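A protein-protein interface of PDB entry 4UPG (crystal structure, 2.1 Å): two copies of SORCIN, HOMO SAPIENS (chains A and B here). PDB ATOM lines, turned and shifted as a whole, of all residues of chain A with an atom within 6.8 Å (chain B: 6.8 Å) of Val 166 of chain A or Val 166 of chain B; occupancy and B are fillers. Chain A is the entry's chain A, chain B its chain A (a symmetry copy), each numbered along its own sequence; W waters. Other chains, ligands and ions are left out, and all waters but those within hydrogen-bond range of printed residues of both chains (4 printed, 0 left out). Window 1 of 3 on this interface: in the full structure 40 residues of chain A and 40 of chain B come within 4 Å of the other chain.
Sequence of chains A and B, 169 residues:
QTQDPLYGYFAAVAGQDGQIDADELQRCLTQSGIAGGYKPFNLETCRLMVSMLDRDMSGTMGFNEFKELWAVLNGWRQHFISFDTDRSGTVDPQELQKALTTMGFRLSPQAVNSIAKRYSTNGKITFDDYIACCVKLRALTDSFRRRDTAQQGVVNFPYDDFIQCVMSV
The backbone carbonyl oxygen (O) of Gln 164 of chain A is in hydrogen-bond range of the side-chain hydroxyl (OG) of Ser 168 of chain A (2.8 Å). The backbone carbonyl oxygen of Gln 164 of chain B sits at hydrogen-bond distance from the side-chain hydroxyl of Ser 168 of chain B (2.8 Å).
Arg 118 of chain A touches Met 167 of chain B, and with the chains exchanged Met 167 of chain A touches Arg 118 of chain B. Lys 136 of chain A touches Met 167 of chain B, and with the chains exchanged Met 167 of chain A touches Lys 136 of chain B. Phe 157 of chain B touches its own counterpart, Phe 157 of chain A. Phe 157 of chain A touches Phe 162 of chain B, and with the chains exchanged Phe 162 of chain A touches Phe 157 of chain B. 15 positions are printed for both chains. Of the 27 pairs that touch across the chains among the printed residues, 27 have their exchanged pair printed and touching as well.
The backbone carbonyl oxygen (O) of Gln 164 of chain B lies within hydrogen-bond range of the side-chain hydroxyl (OG) of Ser 114 of chain A. OG of Ser 114 of chain A is in hydrogen-bond range of OG of Ser 168 of chain B (2.7 Å). The chain-end carboxylate (O) of Val 169 of chain B lies within salt-bridge range of the guanidinium group (NE) of Arg 118 of chain A (2.9 Å). The side-chain amino group (NZ) of Lys 136 of chain A sits at hydrogen-bond distance from the backbone carbonyl oxygen (O) of Val 166 of chain B (3.1 Å). The side-chain amino group (NZ) of Lys 136 of chain A lies within salt-bridge range of the chain-end carboxylate (O) of Val 169 of chain B (2.8 Å). O of Gln 164 of chain A sits at hydrogen-bond distance from OG of Ser 114 of chain B. O of Val 166 of chain A lies within hydrogen-bond range of NZ of Lys 136 of chain B, 3.1 Å away. The side-chain hydroxyl (OG) of Ser 168 of chain A is in hydrogen-bond range of the side-chain hydroxyl (OG) of Ser 114 of chain B (2.7 Å). The chain-end carboxylate of Val 169 of chain A lies within salt-bridge range of the guanidinium group of Arg 118 of chain B, at 2.9 Å. NZ of Lys 136 of chain B is in salt-bridge range of O of Val 169 of chain A.
Of the 15 printed residues of chain A, 11 touch a printed residue of chain B. Hydrophobic or aromatic side chains of chain A that line the printed part of chain B: Leu 140, Phe 157, Phe 162, Val 166 and Met 167. Of the 15 printed residues of chain B, 11 touch a printed residue of chain A. Hydrophobic or aromatic side chains of chain B within 4 Å of the printed part of chain A: Leu 140, Phe 157, Phe 162, Val 166 and Met 167. Among the printed residues, 27 pairs touch across the chains. Among the printed residues, no Asp or Glu carboxylate lies within 4 Å of a Lys or Arg side-chain nitrogen of the other chain.
Water W2 lies within hydrogen-bond range of the side-chain amino group (NZ) of Lys 136 of chain A (2.7 Å), the backbone carbonyl oxygen (O) of Met 167 of chain B (2.8 Å), the chain-end carboxylate (O) of Val 169 of chain B (3.4 Å) and the guanidinium group (NE) of Arg 118 of chain A (3.4 Å). Water W1 lies within hydrogen-bond range of NZ of Lys 136 of chain B (2.7 Å), O of Met 167 of chain A (2.8 Å), O of Val 169 of chain A (3.4 Å) and NE of Arg 118 of chain B (3.4 Å). Water W3 bridges O of Ser 114 of chain B (2.7 Å) and OG of Ser 168 of chain A (3.5 Å). Water W4 lies within hydrogen-bond range of the backbone carbonyl oxygen (O) of Ser 114 of chain A (2.7 Å) and the side-chain hydroxyl (OG) of Ser 168 of chain B (3.5 Å).
CG of Arg 118 of chain A touches O of Met 167 of chain B (3.2 Å). Arg 118 of chain A touches Ser 168 of chain B. Leu 140 of chain A touches Phe 162 of chain B (O to CE2, 3.7 Å). Phe 157 of chain A touches Phe 157 of chain B (CD2 to CD2, 3.8 Å). CE2 of Phe 162 of chain A touches O of Leu 140 of chain B (3.7 Å). Phe 157 of chain B touches Phe 162 of chain A (CE2 to CE1, 3.7 Å). Phe 162 of chain A touches Phe 162 of chain B. CD1 of Leu 140 of chain B touches CG1 of Val 166 of chain A (3.4 Å). Val 166 of chain A touches Val 166 of chain B. CD1 of Leu 140 of chain B touches SD of Met 167 of chain A, 3.98 Å away.
Printed residues of chain B within 4 Å of Phe 157 of chain A: Phe 157 and Phe 162. Asp 161 of chain A touches none of the printed residues of chain B. Of the printed residues of chain B, Gln 164 of chain A touches Ser 114 (2.8 Å). Of the printed residues of chain B, Met 167 of chain A touches Arg 118, Lys 136 and Leu 140. Printed residues of chain A within 4 Å of Phe 157 of chain B: Phe 157 (3.8 Å) and Phe 162 (3.7 Å). Ile 163 of chain B touches none of the printed residues of chain A. Val 166 of chain B touches just these residues of chain A: Lys 136 (3.1 Å), Leu 140 (3.4 Å) and Val 166 (3.0 Å). The nearest residue of chain B that does not touch Val 166 of chain A is Phe 162 of chain B (4.2 Å). The nearest residue of chain A that does not touch Val 166 of chain B is Phe 162 of chain A (4.2 Å). The nearest printed residue of chain A that does not touch Phe 157 of chain B is Val 166 of chain A (7.4 Å).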
ATOM      1  N   SER A 114      21.171 -14.482  27.234  1.00  0.00           N
ATOM      2  CA  SER A 114      21.635 -13.263  26.563  1.00  0.00           C
ATOM      3  C   SER A 114      20.564 -12.155  26.705  1.00  0.00           C
ATOM      4  O   SER A 114      20.862 -10.994  27.044  1.00  0.00           O
ATOM      5  CB  SER A 114      21.937 -13.545  25.080  1.00  0.00           C
ATOM      6  OG  SER A 114      22.218 -12.347  24.333  1.00  0.00           O
ATOM      7  N   ARG A 118      20.375  -8.675  29.036  1.00  0.00           N
ATOM      8  CA  ARG A 118      20.302  -7.464  28.252  1.00  0.00           C
ATOM      9  C   ARG A 118      19.219  -6.521  28.779  1.00  0.00           C
ATOM     10  O   ARG A 118      19.380  -5.315  28.682  1.00  0.00           O
ATOM     11  CB  ARG A 118      20.008  -7.838  26.787  1.00  0.00           C
ATOM     12  CG  ARG A 118      19.645  -6.686  25.885  1.00  0.00           C
ATOM     13  CD  ARG A 118      20.812  -5.726  25.692  1.00  0.00           C
ATOM     14  NE  ARG A 118      20.414  -4.627  24.799  1.00  0.00           N
ATOM     15  CZ  ARG A 118      19.676  -3.594  25.164  1.00  0.00           C
ATOM     16  NH1 ARG A 118      19.250  -3.469  26.417  1.00  0.00           N
ATOM     17  NH2 ARG A 118      19.355  -2.660  24.280  1.00  0.00           N
ATOM     18  N   LYS A 136      12.623  -6.268  18.271  1.00  0.00           N
ATOM     19  CA  LYS A 136      13.956  -6.482  17.734  1.00  0.00           C
ATOM     20  C   LYS A 136      14.095  -7.943  17.343  1.00  0.00           C
ATOM     21  O   LYS A 136      14.632  -8.241  16.277  1.00  0.00           O
ATOM     22  CB  LYS A 136      14.977  -6.012  18.770  1.00  0.00           C
ATOM     23  CG  LYS A 136      16.423  -6.296  18.454  1.00  0.00           C
ATOM     24  CD  LYS A 136      17.371  -5.506  19.398  1.00  0.00           C
ATOM     25  CE  LYS A 136      18.785  -5.952  19.117  1.00  0.00           C
ATOM     26  NZ  LYS A 136      19.796  -5.418  20.052  1.00  0.00           N
ATOM     27  N   LEU A 140      14.897  -8.962  13.506  1.00  0.00           N
ATOM     28  CA  LEU A 140      16.119  -9.729  13.199  1.00  0.00           C
ATOM     29  C   LEU A 140      15.830 -11.108  12.661  1.00  0.00           C
ATOM     30  O   LEU A 140      16.567 -11.595  11.824  1.00  0.00           O
ATOM     31  CB  LEU A 140      16.991  -9.890  14.433  1.00  0.00           C
ATOM     32  CG  LEU A 140      17.606  -8.584  14.900  1.00  0.00           C
ATOM     33  CD1 LEU A 140      18.326  -8.856  16.213  1.00  0.00           C
ATOM     34  CD2 LEU A 140      18.497  -7.991  13.817  1.00  0.00           C
ATOM     35  N   SER A 143      14.856 -10.634   9.152  1.00  0.00           N
ATOM     36  CA  SER A 143      16.075 -10.356   8.362  1.00  0.00           C
ATOM     37  C   SER A 143      16.852 -11.627   8.073  1.00  0.00           C
ATOM     38  O   SER A 143      17.328 -11.863   6.957  1.00  0.00           O
ATOM     39  CB  SER A 143      16.968  -9.339   9.091  1.00  0.00           C
ATOM     40  OG  SER A 143      16.344  -8.072   9.115  1.00  0.00           O
ATOM     41  N   PHE A 157      26.724 -13.893   5.964  1.00  0.00           N
ATOM     42  CA  PHE A 157      26.581 -12.450   6.051  1.00  0.00           C
ATOM     43  C   PHE A 157      27.874 -11.787   5.663  1.00  0.00           C
ATOM     44  O   PHE A 157      28.881 -11.945   6.378  1.00  0.00           O
ATOM     45  CB  PHE A 157      26.327 -12.071   7.503  1.00  0.00           C
ATOM     46  CG  PHE A 157      24.898 -11.933   7.870  1.00  0.00           C
ATOM     47  CD1 PHE A 157      24.200 -10.789   7.535  1.00  0.00           C
ATOM     48  CD2 PHE A 157      24.272 -12.910   8.623  1.00  0.00           C
ATOM     49  CE1 PHE A 157      22.862 -10.626   7.940  1.00  0.00           C
ATOM     50  CE2 PHE A 157      22.942 -12.757   9.012  1.00  0.00           C
ATOM     51  CZ  PHE A 157      22.257 -11.608   8.675  1.00  0.00           C
ATOM     52  N   ASP A 161      26.593  -5.743   4.927  1.00  0.00           N
ATOM     53  CA  ASP A 161      25.193  -6.161   5.020  1.00  0.00           C
ATOM     54  C   ASP A 161      24.797  -6.479   6.486  1.00  0.00           C
ATOM     55  O   ASP A 161      23.732  -6.054   6.965  1.00  0.00           O
ATOM     56  CB  ASP A 161      24.920  -7.363   4.106  1.00  0.00           C
ATOM     57  CG  ASP A 161      23.468  -7.884   4.243  1.00  0.00           C
ATOM     58  OD1 ASP A 161      22.487  -7.094   4.063  1.00  0.00           O
ATOM     59  OD2 ASP A 161      23.288  -9.063   4.628  1.00  0.00           O
ATOM     60  N   PHE A 162      25.679  -7.195   7.203  1.00  0.00           N
ATOM     61  CA  PHE A 162      25.493  -7.476   8.637  1.00  0.00           C
ATOM     62  C   PHE A 162      25.316  -6.167   9.413  1.00  0.00           C
ATOM     63  O   PHE A 162      24.332  -5.980  10.170  1.00  0.00           O
ATOM     64  CB  PHE A 162      26.686  -8.332   9.151  1.00  0.00           C
ATOM     65  CG  PHE A 162      26.692  -8.587  10.635  1.00  0.00           C
ATOM     66  CD1 PHE A 162      25.853  -9.526  11.197  1.00  0.00           C
ATOM     67  CD2 PHE A 162      27.581  -7.917  11.474  1.00  0.00           C
ATOM     68  CE1 PHE A 162      25.859  -9.760  12.560  1.00  0.00           C
ATOM     69  CE2 PHE A 162      27.598  -8.167  12.857  1.00  0.00           C
ATOM     70  CZ  PHE A 162      26.743  -9.079  13.391  1.00  0.00           C
ATOM     71  N   ILE A 163      26.250  -5.242   9.237  1.00  0.00           N
ATOM     72  CA  ILE A 163      26.188  -3.965   9.947  1.00  0.00           C
ATOM     73  C   ILE A 163      24.916  -3.164   9.591  1.00  0.00           C
ATOM     74  O   ILE A 163      24.201  -2.690  10.470  1.00  0.00           O
ATOM     75  CB  ILE A 163      27.425  -3.091   9.655  1.00  0.00           C
ATOM     76  CG1 ILE A 163      28.674  -3.728  10.268  1.00  0.00           C
ATOM     77  CG2 ILE A 163      27.233  -1.679  10.193  1.00  0.00           C
ATOM     78  CD1 ILE A 163      28.632  -3.941  11.780  1.00  0.00           C
ATOM     79  N   GLN A 164      24.663  -3.011   8.308  1.00  0.00           N
ATOM     80  CA  GLN A 164      23.457  -2.339   7.819  1.00  0.00           C
ATOM     81  C   GLN A 164      22.211  -2.867   8.511  1.00  0.00           C
ATOM     82  O   GLN A 164      21.380  -2.133   9.007  1.00  0.00           O
ATOM     83  CB  GLN A 164      23.285  -2.595   6.324  1.00  0.00           C
ATOM     84  CG  GLN A 164      23.556  -1.395   5.467  1.00  0.00           C
ATOM     85  CD  GLN A 164      22.939  -1.548   4.111  1.00  0.00           C
ATOM     86  OE1 GLN A 164      23.498  -2.190   3.242  1.00  0.00           O
ATOM     87  NE2 GLN A 164      21.766  -0.973   3.932  1.00  0.00           N
ATOM     88  N   CYS A 165      22.103  -4.185   8.514  1.00  0.00           N
ATOM     89  CA  CYS A 165      20.949  -4.859   9.026  1.00  0.00           C
ATOM     90  C   CYS A 165      20.819  -4.723  10.553  1.00  0.00           C
ATOM     91  O   CYS A 165      19.768  -4.366  11.096  1.00  0.00           O
ATOM     92  CB  CYS A 165      21.080  -6.313   8.613  1.00  0.00           C
ATOM     93  SG  CYS A 165      19.882  -7.405   9.346  1.00  0.00           S
ATOM     94  N   VAL A 166      21.885  -5.030  11.266  1.00  0.00           N
ATOM     95  CA  VAL A 166      21.801  -5.024  12.694  1.00  0.00           C
ATOM     96  C   VAL A 166      21.780  -3.605  13.272  1.00  0.00           C
ATOM     97  O   VAL A 166      21.122  -3.372  14.259  1.00  0.00           O
ATOM     98  CB  VAL A 166      22.918  -5.871  13.317  1.00  0.00           C
ATOM     99  CG1 VAL A 166      22.795  -5.801  14.832  1.00  0.00           C
ATOM    100  CG2 VAL A 166      22.791  -7.301  12.831  1.00  0.00           C
ATOM    101  N   MET A 167      22.452  -2.642  12.656  1.00  0.00           N
ATOM    102  CA  MET A 167      22.355  -1.241  13.147  1.00  0.00           C
ATOM    103  C   MET A 167      20.976  -0.575  12.924  1.00  0.00           C
ATOM    104  O   MET A 167      20.698   0.422  13.562  1.00  0.00           O
ATOM    105  CB  MET A 167      23.471  -0.353  12.581  1.00  0.00           C
ATOM    106  CG  MET A 167      24.878  -0.823  12.930  1.00  0.00           C
ATOM    107  SD  MET A 167      25.245  -0.664  14.677  1.00  0.00           S
ATOM    108  CE  MET A 167      25.253   1.100  14.948  1.00  0.00           C
ATOM    109  N   SER A 168      20.112  -1.120  12.061  1.00  0.00           N
ATOM    110  CA  SER A 168      18.759  -0.569  11.861  1.00  0.00           C
ATOM    111  C   SER A 168      17.834  -0.871  13.031  1.00  0.00           C
ATOM    112  O   SER A 168      16.828  -0.176  13.216  1.00  0.00           O
ATOM    113  CB  SER A 168      18.101  -1.108  10.589  1.00  0.00           C
ATOM    114  OG  SER A 168      18.884  -0.842   9.454  1.00  0.00           O
ATOM    115  N   VAL A 169      18.146  -1.909  13.811  1.00  0.00           N
ATOM    116  CA  VAL A 169      17.321  -2.237  14.969  1.00  0.00           C
ATOM    117  C   VAL A 169      18.060  -2.083  16.306  1.00  0.00           C
ATOM    118  O   VAL A 169      18.706  -1.079  16.478  1.00  0.00           O
ATOM    119  CB  VAL A 169      16.651  -3.620  14.839  1.00  0.00           C
ATOM    120  CG1 VAL A 169      15.786  -3.630  13.585  1.00  0.00           C
ATOM    121  CG2 VAL A 169      17.669  -4.717  14.727  1.00  0.00           C
ATOM    122  OXT VAL A 169      18.001  -2.889  17.249  1.00  0.00           O
ATOM    123  N   SER B 114      21.694   3.695   6.801  1.00  0.00           N
ATOM    124  CA  SER B 114      21.031   2.867   7.814  1.00  0.00           C
ATOM    125  C   SER B 114      21.214   3.512   9.208  1.00  0.00           C
ATOM    126  O   SER B 114      20.262   3.641  10.002  1.00  0.00           O
ATOM    127  CB  SER B 114      21.598   1.435   7.796  1.00  0.00           C
ATOM    128  OG  SER B 114      21.116   0.633   8.889  1.00  0.00           O
ATOM    129  N   ARG B 118      18.592   5.580  11.743  1.00  0.00           N
ATOM    130  CA  ARG B 118      18.385   4.924  13.012  1.00  0.00           C
ATOM    131  C   ARG B 118      18.489   5.910  14.176  1.00  0.00           C
ATOM    132  O   ARG B 118      17.809   5.731  15.174  1.00  0.00           O
ATOM    133  CB  ARG B 118      19.434   3.807  13.171  1.00  0.00           C
ATOM    134  CG  ARG B 118      19.523   3.194  14.545  1.00  0.00           C
ATOM    135  CD  ARG B 118      18.257   2.430  14.910  1.00  0.00           C
ATOM    136  NE  ARG B 118      18.395   1.843  16.251  1.00  0.00           N
ATOM    137  CZ  ARG B 118      18.269   2.516  17.382  1.00  0.00           C
ATOM    138  NH1 ARG B 118      17.975   3.812  17.375  1.00  0.00           N
ATOM    139  NH2 ARG B 118      18.430   1.900  18.545  1.00  0.00           N
ATOM    140  N   LYS B 136      27.895   0.111  19.822  1.00  0.00           N
ATOM    141  CA  LYS B 136      27.243  -1.019  19.182  1.00  0.00           C
ATOM    142  C   LYS B 136      28.043  -1.409  17.950  1.00  0.00           C
ATOM    143  O   LYS B 136      28.258  -2.597  17.714  1.00  0.00           O
ATOM    144  CB  LYS B 136      25.792  -0.639  18.891  1.00  0.00           C
ATOM    145  CG  LYS B 136      24.993  -1.632  18.087  1.00  0.00           C
ATOM    146  CD  LYS B 136      23.476  -1.299  18.128  1.00  0.00           C
ATOM    147  CE  LYS B 136      22.767  -2.245  17.190  1.00  0.00           C
ATOM    148  NZ  LYS B 136      21.335  -1.947  16.982  1.00  0.00           N
ATOM    149  N   LEU B 140      29.636  -5.119  17.641  1.00  0.00           N
ATOM    150  CA  LEU B 140      29.243  -5.987  16.516  1.00  0.00           C
ATOM    151  C   LEU B 140      30.384  -6.291  15.578  1.00  0.00           C
ATOM    152  O   LEU B 140      30.445  -7.379  15.035  1.00  0.00           O
ATOM    153  CB  LEU B 140      28.131  -5.353  15.696  1.00  0.00           C
ATOM    154  CG  LEU B 140      26.813  -5.272  16.444  1.00  0.00           C
ATOM    155  CD1 LEU B 140      25.836  -4.493  15.576  1.00  0.00           C
ATOM    156  CD2 LEU B 140      26.326  -6.663  16.828  1.00  0.00           C
ATOM    157  N   SER B 143      32.414  -8.848  17.262  1.00  0.00           N
ATOM    158  CA  SER B 143      31.711 -10.144  17.158  1.00  0.00           C
ATOM    159  C   SER B 143      31.894 -10.768  15.787  1.00  0.00           C
ATOM    160  O   SER B 143      32.146 -11.969  15.643  1.00  0.00           O
ATOM    161  CB  SER B 143      30.215  -9.973  17.471  1.00  0.00           C
ATOM    162  OG  SER B 143      30.038  -9.656  18.836  1.00  0.00           O
ATOM    163  N   PHE B 157      26.584 -17.505  10.004  1.00  0.00           N
ATOM    164  CA  PHE B 157      25.930 -17.377  11.294  1.00  0.00           C
ATOM    165  C   PHE B 157      24.803 -18.367  11.394  1.00  0.00           C
ATOM    166  O   PHE B 157      23.817 -18.250  10.644  1.00  0.00           O
ATOM    167  CB  PHE B 157      25.293 -15.997  11.384  1.00  0.00           C
ATOM    168  CG  PHE B 157      26.130 -14.966  12.042  1.00  0.00           C
ATOM    169  CD1 PHE B 157      26.225 -14.921  13.419  1.00  0.00           C
ATOM    170  CD2 PHE B 157      26.756 -13.988  11.289  1.00  0.00           C
ATOM    171  CE1 PHE B 157      26.965 -13.903  14.050  1.00  0.00           C
ATOM    172  CE2 PHE B 157      27.501 -12.988  11.911  1.00  0.00           C
ATOM    173  CZ  PHE B 157      27.586 -12.952  13.287  1.00  0.00           C
ATOM    174  N   ASP B 161      23.058 -18.438  17.367  1.00  0.00           N
ATOM    175  CA  ASP B 161      24.271 -17.652  17.595  1.00  0.00           C
ATOM    176  C   ASP B 161      24.083 -16.181  17.141  1.00  0.00           C
ATOM    177  O   ASP B 161      24.455 -15.239  17.860  1.00  0.00           O
ATOM    178  CB  ASP B 161      25.477 -18.292  16.896  1.00  0.00           C
ATOM    179  CG  ASP B 161      26.763 -17.441  17.049  1.00  0.00           C
ATOM    180  OD1 ASP B 161      27.178 -17.116  18.206  1.00  0.00           O
ATOM    181  OD2 ASP B 161      27.317 -17.002  16.014  1.00  0.00           O
ATOM    182  N   PHE B 162      23.469 -15.993  15.962  1.00  0.00           N
ATOM    183  CA  PHE B 162      23.119 -14.655  15.454  1.00  0.00           C
ATOM    184  C   PHE B 162      22.256 -13.910  16.479  1.00  0.00           C
ATOM    185  O   PHE B 162      22.565 -12.765  16.889  1.00  0.00           O
ATOM    186  CB  PHE B 162      22.431 -14.796  14.066  1.00  0.00           C
ATOM    187  CG  PHE B 162      21.904 -13.511  13.485  1.00  0.00           C
ATOM    188  CD1 PHE B 162      22.753 -12.593  12.905  1.00  0.00           C
ATOM    189  CD2 PHE B 162      20.536 -13.237  13.472  1.00  0.00           C
ATOM    190  CE1 PHE B 162      22.269 -11.414  12.370  1.00  0.00           C
ATOM    191  CE2 PHE B 162      20.043 -12.046  12.915  1.00  0.00           C
ATOM    192  CZ  PHE B 162      20.903 -11.145  12.372  1.00  0.00           C
ATOM    193  N   ILE B 163      21.172 -14.542  16.912  1.00  0.00           N
ATOM    194  CA  ILE B 163      20.268 -13.912  17.873  1.00  0.00           C
ATOM    195  C   ILE B 163      20.974 -13.594  19.210  1.00  0.00           C
ATOM    196  O   ILE B 163      20.885 -12.481  19.722  1.00  0.00           O
ATOM    197  CB  ILE B 163      19.036 -14.795  18.158  1.00  0.00           C
ATOM    198  CG1 ILE B 163      18.154 -14.881  16.911  1.00  0.00           C
ATOM    199  CG2 ILE B 163      18.236 -14.250  19.334  1.00  0.00           C
ATOM    200  CD1 ILE B 163      17.628 -13.548  16.380  1.00  0.00           C
ATOM    201  N   GLN B 164      21.648 -14.580  19.763  1.00  0.00           N
ATOM    202  CA  GLN B 164      22.427 -14.408  20.992  1.00  0.00           C
ATOM    203  C   GLN B 164      23.318 -13.178  20.915  1.00  0.00           C
ATOM    204  O   GLN B 164      23.353 -12.343  21.794  1.00  0.00           O
ATOM    205  CB  GLN B 164      23.339 -15.613  21.206  1.00  0.00           C
ATOM    206  CG  GLN B 164      22.912 -16.505  22.332  1.00  0.00           C
ATOM    207  CD  GLN B 164      24.045 -17.368  22.798  1.00  0.00           C
ATOM    208  OE1 GLN B 164      24.329 -18.393  22.207  1.00  0.00           O
ATOM    209  NE2 GLN B 164      24.711 -16.944  23.853  1.00  0.00           N
ATOM    210  N   CYS B 165      24.057 -13.106  19.820  1.00  0.00           N
ATOM    211  CA  CYS B 165      25.031 -12.077  19.619  1.00  0.00           C
ATOM    212  C   CYS B 165      24.389 -10.691  19.425  1.00  0.00           C
ATOM    213  O   CYS B 165      24.758  -9.700  20.065  1.00  0.00           O
ATOM    214  CB  CYS B 165      25.842 -12.482  18.402  1.00  0.00           C
ATOM    215  SG  CYS B 165      26.961 -11.234  17.806  1.00  0.00           S
ATOM    216  N   VAL B 166      23.436 -10.604  18.521  1.00  0.00           N
ATOM    217  CA  VAL B 166      22.869  -9.326  18.218  1.00  0.00           C
ATOM    218  C   VAL B 166      21.921  -8.832  19.316  1.00  0.00           C
ATOM    219  O   VAL B 166      21.862  -7.651  19.568  1.00  0.00           O
ATOM    220  CB  VAL B 166      22.185  -9.335  16.845  1.00  0.00           C
ATOM    221  CG1 VAL B 166      21.578  -7.962  16.594  1.00  0.00           C
ATOM    222  CG2 VAL B 166      23.209  -9.674  15.779  1.00  0.00           C
ATOM    223  N   MET B 167      21.207  -9.714  20.004  1.00  0.00           N
ATOM    224  CA  MET B 167      20.364  -9.258  21.141  1.00  0.00           C
ATOM    225  C   MET B 167      21.158  -8.769  22.376  1.00  0.00           C
ATOM    226  O   MET B 167      20.587  -8.090  23.208  1.00  0.00           O
ATOM    227  CB  MET B 167      19.335 -10.317  21.557  1.00  0.00           C
ATOM    228  CG  MET B 167      18.366 -10.714  20.449  1.00  0.00           C
ATOM    229  SD  MET B 167      17.246  -9.386  20.003  1.00  0.00           S
ATOM    230  CE  MET B 167      16.239  -9.178  21.462  1.00  0.00           C
ATOM    231  N   SER B 168      22.454  -9.077  22.491  1.00  0.00           N
ATOM    232  CA  SER B 168      23.276  -8.580  23.610  1.00  0.00           C
ATOM    233  C   SER B 168      23.604  -7.101  23.472  1.00  0.00           C
ATOM    234  O   SER B 168      23.926  -6.445  24.471  1.00  0.00           O
ATOM    235  CB  SER B 168      24.594  -9.345  23.738  1.00  0.00           C
ATOM    236  OG  SER B 168      24.375 -10.722  23.898  1.00  0.00           O
ATOM    237  N   VAL B 169      23.549  -6.568  22.249  1.00  0.00           N
ATOM    238  CA  VAL B 169      23.820  -5.149  22.048  1.00  0.00           C
ATOM    239  C   VAL B 169      22.606  -4.363  21.534  1.00  0.00           C
ATOM    240  O   VAL B 169      21.545  -4.550  22.078  1.00  0.00           O
ATOM    241  CB  VAL B 169      25.070  -4.909  21.175  1.00  0.00           C
ATOM    242  CG1 VAL B 169      26.271  -5.562  21.848  1.00  0.00           C
ATOM    243  CG2 VAL B 169      24.908  -5.502  19.806  1.00  0.00           C
ATOM    244  OXT VAL B 169      22.639  -3.508  20.635  1.00  0.00           O
HETATM  245  O   HOH W   1      21.591   0.646  16.188  1.00  0.00           O
HETATM  246  O   HOH W   2      18.656  -6.267  22.377  1.00  0.00           O
HETATM  247  O   HOH W   3      17.832   2.442   9.693  1.00  0.00           O
HETATM  248  O   HOH W   4      23.411 -10.030  27.146  1.00  0.00           O
